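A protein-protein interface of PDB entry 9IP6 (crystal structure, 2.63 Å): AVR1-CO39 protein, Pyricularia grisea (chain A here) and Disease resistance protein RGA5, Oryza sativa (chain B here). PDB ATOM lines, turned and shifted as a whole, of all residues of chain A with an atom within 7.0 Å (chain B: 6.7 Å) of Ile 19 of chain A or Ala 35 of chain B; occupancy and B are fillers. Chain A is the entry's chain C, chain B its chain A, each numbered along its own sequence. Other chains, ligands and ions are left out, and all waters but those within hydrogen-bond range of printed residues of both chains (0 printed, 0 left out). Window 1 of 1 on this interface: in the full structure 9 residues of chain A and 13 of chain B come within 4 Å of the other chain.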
ATOM      1  N   ALA A   2     -26.934  -2.255 -19.825  1.00  0.00           N
ATOM      2  CA  ALA A   2     -26.585  -3.350 -20.715  1.00  0.00           C
ATOM      3  C   ALA A   2     -25.996  -2.801 -22.018  1.00  0.00           C
ATOM      4  O   ALA A   2     -26.668  -2.774 -23.064  1.00  0.00           O
ATOM      5  CB  ALA A   2     -27.807  -4.216 -20.996  1.00  0.00           C
ATOM      6  N   TRP A   3     -24.748  -2.337 -21.949  1.00  0.00           N
ATOM      7  CA  TRP A   3     -24.055  -1.938 -23.163  1.00  0.00           C
ATOM      8  C   TRP A   3     -23.398  -3.119 -23.866  1.00  0.00           C
ATOM      9  O   TRP A   3     -23.075  -3.012 -25.048  1.00  0.00           O
ATOM     10  CB  TRP A   3     -23.013  -0.863 -22.853  1.00  0.00           C
ATOM     11  CG  TRP A   3     -21.749  -1.381 -22.273  1.00  0.00           C
ATOM     12  CD1 TRP A   3     -21.598  -2.040 -21.082  1.00  0.00           C
ATOM     13  CD2 TRP A   3     -20.443  -1.270 -22.841  1.00  0.00           C
ATOM     14  NE1 TRP A   3     -20.271  -2.359 -20.883  1.00  0.00           N
ATOM     15  CE2 TRP A   3     -19.542  -1.898 -21.951  1.00  0.00           C
ATOM     16  CE3 TRP A   3     -19.944  -0.712 -24.020  1.00  0.00           C
ATOM     17  CZ2 TRP A   3     -18.177  -1.980 -22.207  1.00  0.00           C
ATOM     18  CZ3 TRP A   3     -18.585  -0.791 -24.268  1.00  0.00           C
ATOM     19  CH2 TRP A   3     -17.718  -1.419 -23.364  1.00  0.00           C
ATOM     20  N   LYS A   4     -23.189  -4.234 -23.168  1.00  0.00           N
ATOM     21  CA  LYS A   4     -22.754  -5.475 -23.787  1.00  0.00           C
ATOM     22  C   LYS A   4     -23.682  -6.606 -23.357  1.00  0.00           C
ATOM     23  O   LYS A   4     -24.282  -6.565 -22.279  1.00  0.00           O
ATOM     24  CB  LYS A   4     -21.288  -5.798 -23.448  1.00  0.00           C
ATOM     25  CG  LYS A   4     -20.292  -4.955 -24.237  1.00  0.00           C
ATOM     26  CD  LYS A   4     -18.900  -5.567 -24.235  1.00  0.00           C
ATOM     27  CE  LYS A   4     -17.905  -4.772 -25.076  1.00  0.00           C
ATOM     28  NZ  LYS A   4     -16.535  -5.391 -25.047  1.00  0.00           N
ATOM     29  N   CYS A   6     -23.228  -9.757 -22.460  1.00  0.00           N
ATOM     30  CA  CYS A   6     -22.874 -10.825 -21.537  1.00  0.00           C
ATOM     31  C   CYS A   6     -22.059 -10.301 -20.369  1.00  0.00           C
ATOM     32  O   CYS A   6     -21.325  -9.313 -20.480  1.00  0.00           O
ATOM     33  CB  CYS A   6     -22.071 -11.951 -22.236  1.00  0.00           C
ATOM     34  SG  CYS A   6     -22.808 -12.525 -23.789  1.00  0.00           S
ATOM     35  N   ILE A   7     -22.186 -11.005 -19.254  1.00  0.00           N
ATOM     36  CA  ILE A   7     -21.326 -10.843 -18.095  1.00  0.00           C
ATOM     37  C   ILE A   7     -20.669 -12.190 -17.844  1.00  0.00           C
ATOM     38  O   ILE A   7     -21.360 -13.204 -17.682  1.00  0.00           O
ATOM     39  CB  ILE A   7     -22.112 -10.370 -16.861  1.00  0.00           C
ATOM     40  CG1 ILE A   7     -22.304  -8.855 -16.904  1.00  0.00           C
ATOM     41  CG2 ILE A   7     -21.422 -10.815 -15.575  1.00  0.00           C
ATOM     42  CD1 ILE A   7     -23.213  -8.332 -15.811  1.00  0.00           C
ATOM     43  N   ILE A   8     -19.343 -12.209 -17.837  1.00  0.00           N
ATOM     44  CA  ILE A   8     -18.598 -13.406 -17.492  1.00  0.00           C
ATOM     45  C   ILE A   8     -18.162 -13.284 -16.043  1.00  0.00           C
ATOM     46  O   ILE A   8     -17.445 -12.346 -15.669  1.00  0.00           O
ATOM     47  CB  ILE A   8     -17.395 -13.615 -18.421  1.00  0.00           C
ATOM     48  CG1 ILE A   8     -17.836 -13.646 -19.898  1.00  0.00           C
ATOM     49  CG2 ILE A   8     -16.696 -14.898 -18.051  1.00  0.00           C
ATOM     50  CD1 ILE A   8     -18.826 -14.772 -20.268  1.00  0.00           C
ATOM     51  N   GLN A   9     -18.605 -14.217 -15.217  1.00  0.00           N
ATOM     52  CA  GLN A   9     -18.190 -14.241 -13.826  1.00  0.00           C
ATOM     53  C   GLN A   9     -17.041 -15.218 -13.625  1.00  0.00           C
ATOM     54  O   GLN A   9     -16.949 -16.256 -14.291  1.00  0.00           O
ATOM     55  CB  GLN A   9     -19.365 -14.606 -12.929  1.00  0.00           C
ATOM     56  CG  GLN A   9     -20.410 -13.513 -12.860  1.00  0.00           C
ATOM     57  CD  GLN A   9     -21.472 -13.836 -11.854  1.00  0.00           C
ATOM     58  OE1 GLN A   9     -21.171 -14.372 -10.789  1.00  0.00           O
ATOM     59  NE2 GLN A   9     -22.734 -13.538 -12.188  1.00  0.00           N
ATOM     60  N   ARG A  10     -16.147 -14.861 -12.709  1.00  0.00           N
ATOM     61  CA  ARG A  10     -14.910 -15.600 -12.494  1.00  0.00           C
ATOM     62  C   ARG A  10     -14.784 -15.955 -11.015  1.00  0.00           C
ATOM     63  O   ARG A  10     -14.618 -15.072 -10.159  1.00  0.00           O
ATOM     64  CB  ARG A  10     -13.725 -14.783 -12.983  1.00  0.00           C
ATOM     65  CG  ARG A  10     -12.397 -15.359 -12.622  1.00  0.00           C
ATOM     66  CD  ARG A  10     -11.355 -14.535 -13.283  1.00  0.00           C
ATOM     67  NE  ARG A  10     -10.049 -15.155 -13.196  1.00  0.00           N
ATOM     68  CZ  ARG A  10      -9.071 -14.706 -12.423  1.00  0.00           C
ATOM     69  NH1 ARG A  10      -9.270 -13.625 -11.680  1.00  0.00           N
ATOM     70  NH2 ARG A  10      -7.900 -15.337 -12.407  1.00  0.00           N
ATOM     71  N   VAL A  16     -16.601 -15.145  -6.248  1.00  0.00           N
ATOM     72  CA  VAL A  16     -16.521 -14.338  -7.458  1.00  0.00           C
ATOM     73  C   VAL A  16     -16.098 -12.931  -7.048  1.00  0.00           C
ATOM     74  O   VAL A  16     -16.842 -12.214  -6.371  1.00  0.00           O
ATOM     75  CB  VAL A  16     -17.850 -14.321  -8.213  1.00  0.00           C
ATOM     76  CG1 VAL A  16     -17.753 -13.393  -9.441  1.00  0.00           C
ATOM     77  CG2 VAL A  16     -18.234 -15.748  -8.602  1.00  0.00           C
ATOM     78  N   ASN A  17     -14.883 -12.545  -7.438  1.00  0.00           N
ATOM     79  CA  ASN A  17     -14.341 -11.232  -7.132  1.00  0.00           C
ATOM     80  C   ASN A  17     -14.039 -10.433  -8.381  1.00  0.00           C
ATOM     81  O   ASN A  17     -13.510  -9.317  -8.281  1.00  0.00           O
ATOM     82  CB  ASN A  17     -13.075 -11.363  -6.276  1.00  0.00           C
ATOM     83  CG  ASN A  17     -13.394 -11.786  -4.866  1.00  0.00           C
ATOM     84  OD1 ASN A  17     -14.411 -11.369  -4.324  1.00  0.00           O
ATOM     85  ND2 ASN A  17     -12.556 -12.642  -4.278  1.00  0.00           N
ATOM     86  N   ASN A  18     -14.364 -10.976  -9.548  1.00  0.00           N
ATOM     87  CA  ASN A  18     -14.005 -10.396 -10.826  1.00  0.00           C
ATOM     88  C   ASN A  18     -15.117 -10.720 -11.796  1.00  0.00           C
ATOM     89  O   ASN A  18     -15.617 -11.845 -11.803  1.00  0.00           O
ATOM     90  CB  ASN A  18     -12.678 -10.950 -11.334  1.00  0.00           C
ATOM     91  CG  ASN A  18     -11.538 -10.581 -10.442  1.00  0.00           C
ATOM     92  OD1 ASN A  18     -10.944  -9.521 -10.595  1.00  0.00           O
ATOM     93  ND2 ASN A  18     -11.239 -11.437  -9.479  1.00  0.00           N
ATOM     94  N   ILE A  19     -15.542  -9.734 -12.578  1.00  0.00           N
ATOM     95  CA  ILE A  19     -16.465 -10.013 -13.662  1.00  0.00           C
ATOM     96  C   ILE A  19     -16.065  -9.157 -14.849  1.00  0.00           C
ATOM     97  O   ILE A  19     -15.466  -8.085 -14.701  1.00  0.00           O
ATOM     98  CB  ILE A  19     -17.958  -9.819 -13.297  1.00  0.00           C
ATOM     99  CG1 ILE A  19     -18.387  -8.375 -13.306  1.00  0.00           C
ATOM    100  CG2 ILE A  19     -18.301 -10.411 -11.947  1.00  0.00           C
ATOM    101  CD1 ILE A  19     -19.880  -8.330 -13.086  1.00  0.00           C
ATOM    102  N   TYR A  20     -16.349  -9.686 -16.036  1.00  0.00           N
ATOM    103  CA  TYR A  20     -15.916  -9.105 -17.289  1.00  0.00           C
ATOM    104  C   TYR A  20     -17.129  -9.020 -18.205  1.00  0.00           C
ATOM    105  O   TYR A  20     -18.051  -9.835 -18.112  1.00  0.00           O
ATOM    106  CB  TYR A  20     -14.767  -9.945 -17.907  1.00  0.00           C
ATOM    107  CG  TYR A  20     -13.639 -10.220 -16.920  1.00  0.00           C
ATOM    108  CD1 TYR A  20     -13.738 -11.248 -15.983  1.00  0.00           C
ATOM    109  CD2 TYR A  20     -12.485  -9.438 -16.914  1.00  0.00           C
ATOM    110  CE1 TYR A  20     -12.723 -11.487 -15.067  1.00  0.00           C
ATOM    111  CE2 TYR A  20     -11.465  -9.668 -16.004  1.00  0.00           C
ATOM    112  CZ  TYR A  20     -11.585 -10.688 -15.076  1.00  0.00           C
ATOM    113  OH  TYR A  20     -10.564 -10.904 -14.162  1.00  0.00           O
ATOM    114  N   THR A  21     -17.151  -8.005 -19.057  1.00  0.00           N
ATOM    115  CA  THR A  21     -18.201  -7.895 -20.055  1.00  0.00           C
ATOM    116  C   THR A  21     -17.750  -8.443 -21.411  1.00  0.00           C
ATOM    117  O   THR A  21     -16.559  -8.551 -21.718  1.00  0.00           O
ATOM    118  CB  THR A  21     -18.648  -6.447 -20.193  1.00  0.00           C
ATOM    119  OG1 THR A  21     -17.510  -5.643 -20.510  1.00  0.00           O
ATOM    120  CG2 THR A  21     -19.285  -5.974 -18.882  1.00  0.00           C
ATOM    121  N   ILE A  30      -8.835 -12.260 -20.036  1.00  0.00           N
ATOM    122  CA  ILE A  30      -8.983 -12.257 -18.592  1.00  0.00           C
ATOM    123  C   ILE A  30      -7.619 -12.617 -18.039  1.00  0.00           C
ATOM    124  O   ILE A  30      -7.159 -13.753 -18.207  1.00  0.00           O
ATOM    125  CB  ILE A  30     -10.060 -13.231 -18.104  1.00  0.00           C
ATOM    126  CG1 ILE A  30     -11.449 -12.751 -18.551  1.00  0.00           C
ATOM    127  CG2 ILE A  30      -9.983 -13.370 -16.594  1.00  0.00           C
ATOM    128  CD1 ILE A  30     -12.563 -13.778 -18.343  1.00  0.00           C
ATOM    129  N   THR A  59     -26.578 -10.076 -19.537  1.00  0.00           N
ATOM    130  CA  THR A  59     -26.356  -9.107 -18.466  1.00  0.00           C
ATOM    131  C   THR A  59     -27.544  -9.021 -17.511  1.00  0.00           C
ATOM    132  O   THR A  59     -27.359  -9.030 -16.290  1.00  0.00           O
ATOM    133  CB  THR A  59     -26.040  -7.734 -19.058  1.00  0.00           C
ATOM    134  OG1 THR A  59     -24.873  -7.830 -19.893  1.00  0.00           O
ATOM    135  CG2 THR A  59     -25.793  -6.717 -17.937  1.00  0.00           C
ATOM    136  N   TYR A  62     -27.922 -11.291 -14.680  1.00  0.00           N
ATOM    137  CA  TYR A  62     -26.755 -11.184 -13.776  1.00  0.00           C
ATOM    138  C   TYR A  62     -25.855 -12.461 -13.804  1.00  0.00           C
ATOM    139  O   TYR A  62     -25.044 -12.657 -14.719  1.00  0.00           O
ATOM    140  CB  TYR A  62     -27.178 -10.893 -12.327  1.00  0.00           C
ATOM    141  CG  TYR A  62     -28.419 -10.023 -12.131  1.00  0.00           C
ATOM    142  CD1 TYR A  62     -29.352 -10.339 -11.147  1.00  0.00           C
ATOM    143  CD2 TYR A  62     -28.647  -8.882 -12.900  1.00  0.00           C
ATOM    144  CE1 TYR A  62     -30.490  -9.568 -10.944  1.00  0.00           C
ATOM    145  CE2 TYR A  62     -29.785  -8.098 -12.699  1.00  0.00           C
ATOM    146  CZ  TYR A  62     -30.698  -8.454 -11.721  1.00  0.00           C
ATOM    147  OH  TYR A  62     -31.823  -7.698 -11.510  1.00  0.00           O
ATOM    148  N   ALA B  28     -22.309  -9.198  -5.082  1.00  0.00           N
ATOM    149  CA  ALA B  28     -22.681  -9.710  -6.395  1.00  0.00           C
ATOM    150  C   ALA B  28     -23.588  -8.728  -7.132  1.00  0.00           C
ATOM    151  O   ALA B  28     -23.488  -8.582  -8.354  1.00  0.00           O
ATOM    152  CB  ALA B  28     -23.349 -11.082  -6.264  1.00  0.00           C
ATOM    153  N   ALA B  30     -23.613  -5.360  -6.711  1.00  0.00           N
ATOM    154  CA  ALA B  30     -22.774  -4.244  -7.122  1.00  0.00           C
ATOM    155  C   ALA B  30     -21.896  -4.608  -8.325  1.00  0.00           C
ATOM    156  O   ALA B  30     -21.780  -3.813  -9.270  1.00  0.00           O
ATOM    157  CB  ALA B  30     -21.926  -3.771  -5.938  1.00  0.00           C
ATOM    158  N   LEU B  31     -21.259  -5.793  -8.308  1.00  0.00           N
ATOM    159  CA  LEU B  31     -20.414  -6.206  -9.437  1.00  0.00           C
ATOM    160  C   LEU B  31     -21.186  -6.150 -10.745  1.00  0.00           C
ATOM    161  O   LEU B  31     -20.742  -5.513 -11.711  1.00  0.00           O
ATOM    162  CB  LEU B  31     -19.857  -7.611  -9.219  1.00  0.00           C
ATOM    163  CG  LEU B  31     -18.604  -7.734  -8.343  1.00  0.00           C
ATOM    164  CD1 LEU B  31     -18.253  -9.190  -8.092  1.00  0.00           C
ATOM    165  CD2 LEU B  31     -17.432  -6.991  -8.955  1.00  0.00           C
ATOM    166  N   ALA B  32     -22.361  -6.797 -10.779  1.00  0.00           N
ATOM    167  CA  ALA B  32     -23.241  -6.787 -11.945  1.00  0.00           C
ATOM    168  C   ALA B  32     -23.712  -5.383 -12.299  1.00  0.00           C
ATOM    169  O   ALA B  32     -23.872  -5.060 -13.484  1.00  0.00           O
ATOM    170  CB  ALA B  32     -24.452  -7.688 -11.690  1.00  0.00           C
ATOM    171  N   LEU B  33     -23.958  -4.536 -11.293  1.00  0.00           N
ATOM    172  CA  LEU B  33     -24.487  -3.210 -11.581  1.00  0.00           C
ATOM    173  C   LEU B  33     -23.437  -2.322 -12.229  1.00  0.00           C
ATOM    174  O   LEU B  33     -23.734  -1.604 -13.191  1.00  0.00           O
ATOM    175  CB  LEU B  33     -25.015  -2.574 -10.304  1.00  0.00           C
ATOM    176  CG  LEU B  33     -26.502  -2.761 -10.059  1.00  0.00           C
ATOM    177  CD1 LEU B  33     -26.791  -2.180  -8.694  1.00  0.00           C
ATOM    178  CD2 LEU B  33     -27.329  -2.074 -11.131  1.00  0.00           C
ATOM    179  N   ALA B  34     -22.210  -2.338 -11.703  1.00  0.00           N
ATOM    180  CA  ALA B  34     -21.125  -1.597 -12.344  1.00  0.00           C
ATOM    181  C   ALA B  34     -20.895  -2.099 -13.756  1.00  0.00           C
ATOM    182  O   ALA B  34     -20.753  -1.298 -14.688  1.00  0.00           O
ATOM    183  CB  ALA B  34     -19.834  -1.707 -11.530  1.00  0.00           C
ATOM    184  N   ALA B  35     -20.870  -3.429 -13.933  1.00  0.00           N
ATOM    185  CA  ALA B  35     -20.626  -4.021 -15.252  1.00  0.00           C
ATOM    186  C   ALA B  35     -21.615  -3.523 -16.300  1.00  0.00           C
ATOM    187  O   ALA B  35     -21.263  -3.423 -17.481  1.00  0.00           O
ATOM    188  CB  ALA B  35     -20.675  -5.546 -15.160  1.00  0.00           C
ATOM    189  N   SER B  36     -22.841  -3.177 -15.888  1.00  0.00           N
ATOM    190  CA  SER B  36     -23.863  -2.733 -16.826  1.00  0.00           C
ATOM    191  C   SER B  36     -23.547  -1.393 -17.470  1.00  0.00           C
ATOM    192  O   SER B  36     -24.169  -1.063 -18.484  1.00  0.00           O
ATOM    193  CB  SER B  36     -25.227  -2.647 -16.133  1.00  0.00           C
ATOM    194  OG  SER B  36     -25.291  -1.532 -15.260  1.00  0.00           O
ATOM    195  N   VAL B  37     -22.593  -0.637 -16.940  1.00  0.00           N
ATOM    196  CA  VAL B  37     -22.368   0.751 -17.334  1.00  0.00           C
ATOM    197  C   VAL B  37     -21.429   0.829 -18.539  1.00  0.00           C
ATOM    198  O   VAL B  37     -20.411   0.132 -18.604  1.00  0.00           O
ATOM    199  CB  VAL B  37     -21.837   1.543 -16.119  1.00  0.00           C
ATOM    200  CG1 VAL B  37     -21.206   2.872 -16.512  1.00  0.00           C
ATOM    201  CG2 VAL B  37     -22.968   1.755 -15.105  1.00  0.00           C
ATOM    202  N   ASN B  38     -21.767   1.699 -19.494  1.00  0.00           N
ATOM    203  CA  ASN B  38     -21.038   1.786 -20.759  1.00  0.00           C
ATOM    204  C   ASN B  38     -19.545   1.968 -20.547  1.00  0.00           C
ATOM    205  O   ASN B  38     -19.113   2.829 -19.778  1.00  0.00           O
ATOM    206  CB  ASN B  38     -21.574   2.944 -21.601  1.00  0.00           C
ATOM    207  CG  ASN B  38     -23.049   2.821 -21.865  1.00  0.00           C
ATOM    208  OD1 ASN B  38     -23.867   3.187 -21.021  1.00  0.00           O
ATOM    209  ND2 ASN B  38     -23.406   2.293 -23.028  1.00  0.00           N
ATOM    210  N   GLY B  39     -18.755   1.162 -21.249  1.00  0.00           N
ATOM    211  CA  GLY B  39     -17.318   1.249 -21.175  1.00  0.00           C
ATOM    212  C   GLY B  39     -16.665   0.346 -20.150  1.00  0.00           C
ATOM    213  O   GLY B  39     -15.433   0.222 -20.160  1.00  0.00           O
ATOM    214  N   VAL B  40     -17.434  -0.287 -19.266  1.00  0.00           N
ATOM    215  CA  VAL B  40     -16.834  -1.162 -18.266  1.00  0.00           C
ATOM    216  C   VAL B  40     -16.396  -2.456 -18.934  1.00  0.00           C
ATOM    217  O   VAL B  40     -17.208  -3.147 -19.559  1.00  0.00           O
ATOM    218  CB  VAL B  40     -17.813  -1.447 -17.124  1.00  0.00           C
ATOM    219  CG1 VAL B  40     -17.219  -2.501 -16.187  1.00  0.00           C
ATOM    220  CG2 VAL B  40     -18.171  -0.141 -16.388  1.00  0.00           C
ATOM    221  N   ASP B  41     -15.109  -2.789 -18.806  1.00  0.00           N
ATOM    222  CA  ASP B  41     -14.638  -4.114 -19.200  1.00  0.00           C
ATOM    223  C   ASP B  41     -14.541  -5.065 -18.023  1.00  0.00           C
ATOM    224  O   ASP B  41     -14.909  -6.231 -18.151  1.00  0.00           O
ATOM    225  CB  ASP B  41     -13.270  -4.038 -19.883  1.00  0.00           C
ATOM    226  CG  ASP B  41     -13.297  -3.211 -21.131  1.00  0.00           C
ATOM    227  OD1 ASP B  41     -14.342  -3.202 -21.813  1.00  0.00           O
ATOM    228  OD2 ASP B  41     -12.277  -2.557 -21.426  1.00  0.00           O
ATOM    229  N   SER B  42     -14.048  -4.600 -16.878  1.00  0.00           N
ATOM    230  CA  SER B  42     -13.919  -5.460 -15.714  1.00  0.00           C
ATOM    231  C   SER B  42     -14.286  -4.690 -14.449  1.00  0.00           C
ATOM    232  O   SER B  42     -14.179  -3.460 -14.379  1.00  0.00           O
ATOM    233  CB  SER B  42     -12.501  -6.032 -15.587  1.00  0.00           C
ATOM    234  OG  SER B  42     -11.525  -5.002 -15.706  1.00  0.00           O
ATOM    235  N   VAL B  43     -14.744  -5.446 -13.453  1.00  0.00           N
ATOM    236  CA  VAL B  43     -15.029  -4.952 -12.120  1.00  0.00           C
ATOM    237  C   VAL B  43     -14.413  -5.914 -11.118  1.00  0.00           C
ATOM    238  O   VAL B  43     -14.549  -7.133 -11.247  1.00  0.00           O
ATOM    239  CB  VAL B  43     -16.544  -4.812 -11.884  1.00  0.00           C
ATOM    240  CG1 VAL B  43     -16.812  -3.973 -10.611  1.00  0.00           C
ATOM    241  CG2 VAL B  43     -17.203  -4.173 -13.083  1.00  0.00           C
ATOM    242  N   GLU B  44     -13.755  -5.371 -10.104  1.00  0.00           N
ATOM    243  CA  GLU B  44     -13.106  -6.199  -9.100  1.00  0.00           C
ATOM    244  C   GLU B  44     -13.509  -5.755  -7.700  1.00  0.00           C
ATOM    245  O   GLU B  44     -13.813  -4.584  -7.471  1.00  0.00           O
ATOM    246  CB  GLU B  44     -11.594  -6.132  -9.269  1.00  0.00           C
ATOM    247  CG  GLU B  44     -10.810  -7.152  -8.488  1.00  0.00           C
ATOM    248  CD  GLU B  44      -9.363  -6.724  -8.339  1.00  0.00           C
ATOM    249  OE1 GLU B  44      -8.633  -7.351  -7.538  1.00  0.00           O
ATOM    250  OE2 GLU B  44      -8.967  -5.738  -9.010  1.00  0.00           O
ATOM    251  N   VAL B  55     -13.140  -0.529 -11.108  1.00  0.00           N
ATOM    252  CA  VAL B  55     -13.840  -0.609 -12.383  1.00  0.00           C
ATOM    253  C   VAL B  55     -12.877  -0.158 -13.468  1.00  0.00           C
ATOM    254  O   VAL B  55     -12.320   0.947 -13.384  1.00  0.00           O
ATOM    255  CB  VAL B  55     -15.116   0.253 -12.372  1.00  0.00           C
ATOM    256  CG1 VAL B  55     -15.806   0.229 -13.725  1.00  0.00           C
ATOM    257  CG2 VAL B  55     -16.067  -0.199 -11.253  1.00  0.00           C
ATOM    258  N   LEU B  65     -21.703   6.121 -13.052  1.00  0.00           N
ATOM    259  CA  LEU B  65     -21.365   4.867 -12.377  1.00  0.00           C
ATOM    260  C   LEU B  65     -21.642   4.935 -10.878  1.00  0.00           C
ATOM    261  O   LEU B  65     -22.278   4.037 -10.308  1.00  0.00           O
ATOM    262  CB  LEU B  65     -19.894   4.525 -12.609  1.00  0.00           C
ATOM    263  CG  LEU B  65     -19.339   3.350 -11.787  1.00  0.00           C
ATOM    264  CD1 LEU B  65     -19.992   2.051 -12.201  1.00  0.00           C
ATOM    265  CD2 LEU B  65     -17.821   3.255 -11.915  1.00  0.00           C
ATOM    266  N   LEU B  68     -25.405   5.226  -9.935  1.00  0.00           N
ATOM    267  CA  LEU B  68     -26.128   3.959 -10.017  1.00  0.00           C
ATOM    268  C   LEU B  68     -25.851   3.091  -8.798  1.00  0.00           C
ATOM    269  O   LEU B  68     -26.778   2.559  -8.176  1.00  0.00           O
ATOM    270  CB  LEU B  68     -25.752   3.215 -11.302  1.00  0.00           C
ATOM    271  CG  LEU B  68     -26.297   1.785 -11.435  1.00  0.00           C
ATOM    272  CD1 LEU B  68     -27.796   1.773 -11.705  1.00  0.00           C
ATOM    273  CD2 LEU B  68     -25.571   1.040 -12.501  1.00  0.00           C
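The backbone carbonyl oxygen of Ser 36 of chain B is in hydrogen-bond range of the backbone NH of Ala 2 of chain A, at 3.3 Å. O of Val 37 of chain B sits at hydrogen-bond distance from NE1 of Trp 3 of chain A. O of Val 40 of chain B lies close to NE1 of Trp 3 of chain A (3.4 Å). The backbone carbonyl oxygen (O) of Val 40 of chain B is in hydrogen-bond range of the side-chain hydroxyl (OG1) of Thr 21 of chain A, at 2.7 Å. The backbone NH (N) of Thr 21 of chain A sits at hydrogen-bond distance from the backbone carbonyl oxygen (O) of Asp 41 of chain B (3.0 Å). N of Val 43 of chain B lies within hydrogen-bond range of O of Ile 19 of chain A (3.0 Å).
OG of Ser 36 of chain B sits at hydrogen-bond distance from O of Leu 33 of chain B (2.6 Å). The backbone NH (N) of Ile 8 of chain A lies within hydrogen-bond range of the backbone carbonyl oxygen (O) of Tyr 20 of chain A. The backbone NH (N) of Arg 10 of chain A is in hydrogen-bond range of the backbone carbonyl oxygen (O) of Asn 18 of chain A.
Among the printed residues, pairs that only touch across the chains: Trp 3 of chain A with Ala 35 of chain B, Trp 3 of chain A with Ser 36 of chain B, Trp 3 of chain A with Asn 38 of chain B, Trp 3 of chain A with Gly 39 of chain B, Ile 7 of chain A with Ala 35 of chain B, Val 16 of chain A with Leu 31 of chain B, Asn 17 of chain A with Val 43 of chain B, Asn 17 of chain A with Glu 44 of chain B, Asn 18 of chain A with Val 43 of chain B, Asn 18 of chain A with Glu 44 of chain B, Ile 19 of chain A with Leu 31 of chain B, Ile 19 of chain A with Ala 32 of chain B, Ile 19 of chain A with Ala 35 of chain B, Ile 19 of chain A with Asp 41 of chain B, Ile 19 of chain A with Ser 42 of chain B, Tyr 20 of chain A with Asp 41 of chain B, Tyr 20 of chain A with Ser 42 of chain B and Thr 21 of chain A with Ala 35 of chain B.
Ile 19 of chain A touches six residues of chain B. Of chain A, only Trp 3 (3.7 Å), Ile 7 (3.8 Å), Ile 19 (3.6 Å) and Thr 21 (3.5 Å) come within 4 Å of Ala 35 of chain B. Printed residues of chain B within 4 Å of Ala 2 of chain A: Ser 36 (3.3 Å). Of the printed residues of chain A, Asn 38 of chain B touches Trp 3. Of the printed residues of chain A, Leu 31 of chain B touches Val 16 and Ile 19. Ile 8 of chain A touches none of the printed residues of chain B. The nearest residue of chain A that does not touch Ala 35 of chain B is Thr 59 of chain A (5.5 Å). The nearest printed residue of chain B that does not touch Tyr 20 of chain A is Val 43 of chain B (5.2 Å).
Hydrophobic or aromatic side chains of chain B within 4 Å of the printed part of chain A: Leu 31 and Ala 35. Of the 17 printed residues of chain A, 9 touch a printed residue of chain B. Hydrophobic or aromatic side chains of chain A that line the printed part of chain B: Trp 3, Ile 7, Ile 19 and Tyr 20. Among the printed residues, 24 pairs touch across the chains.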
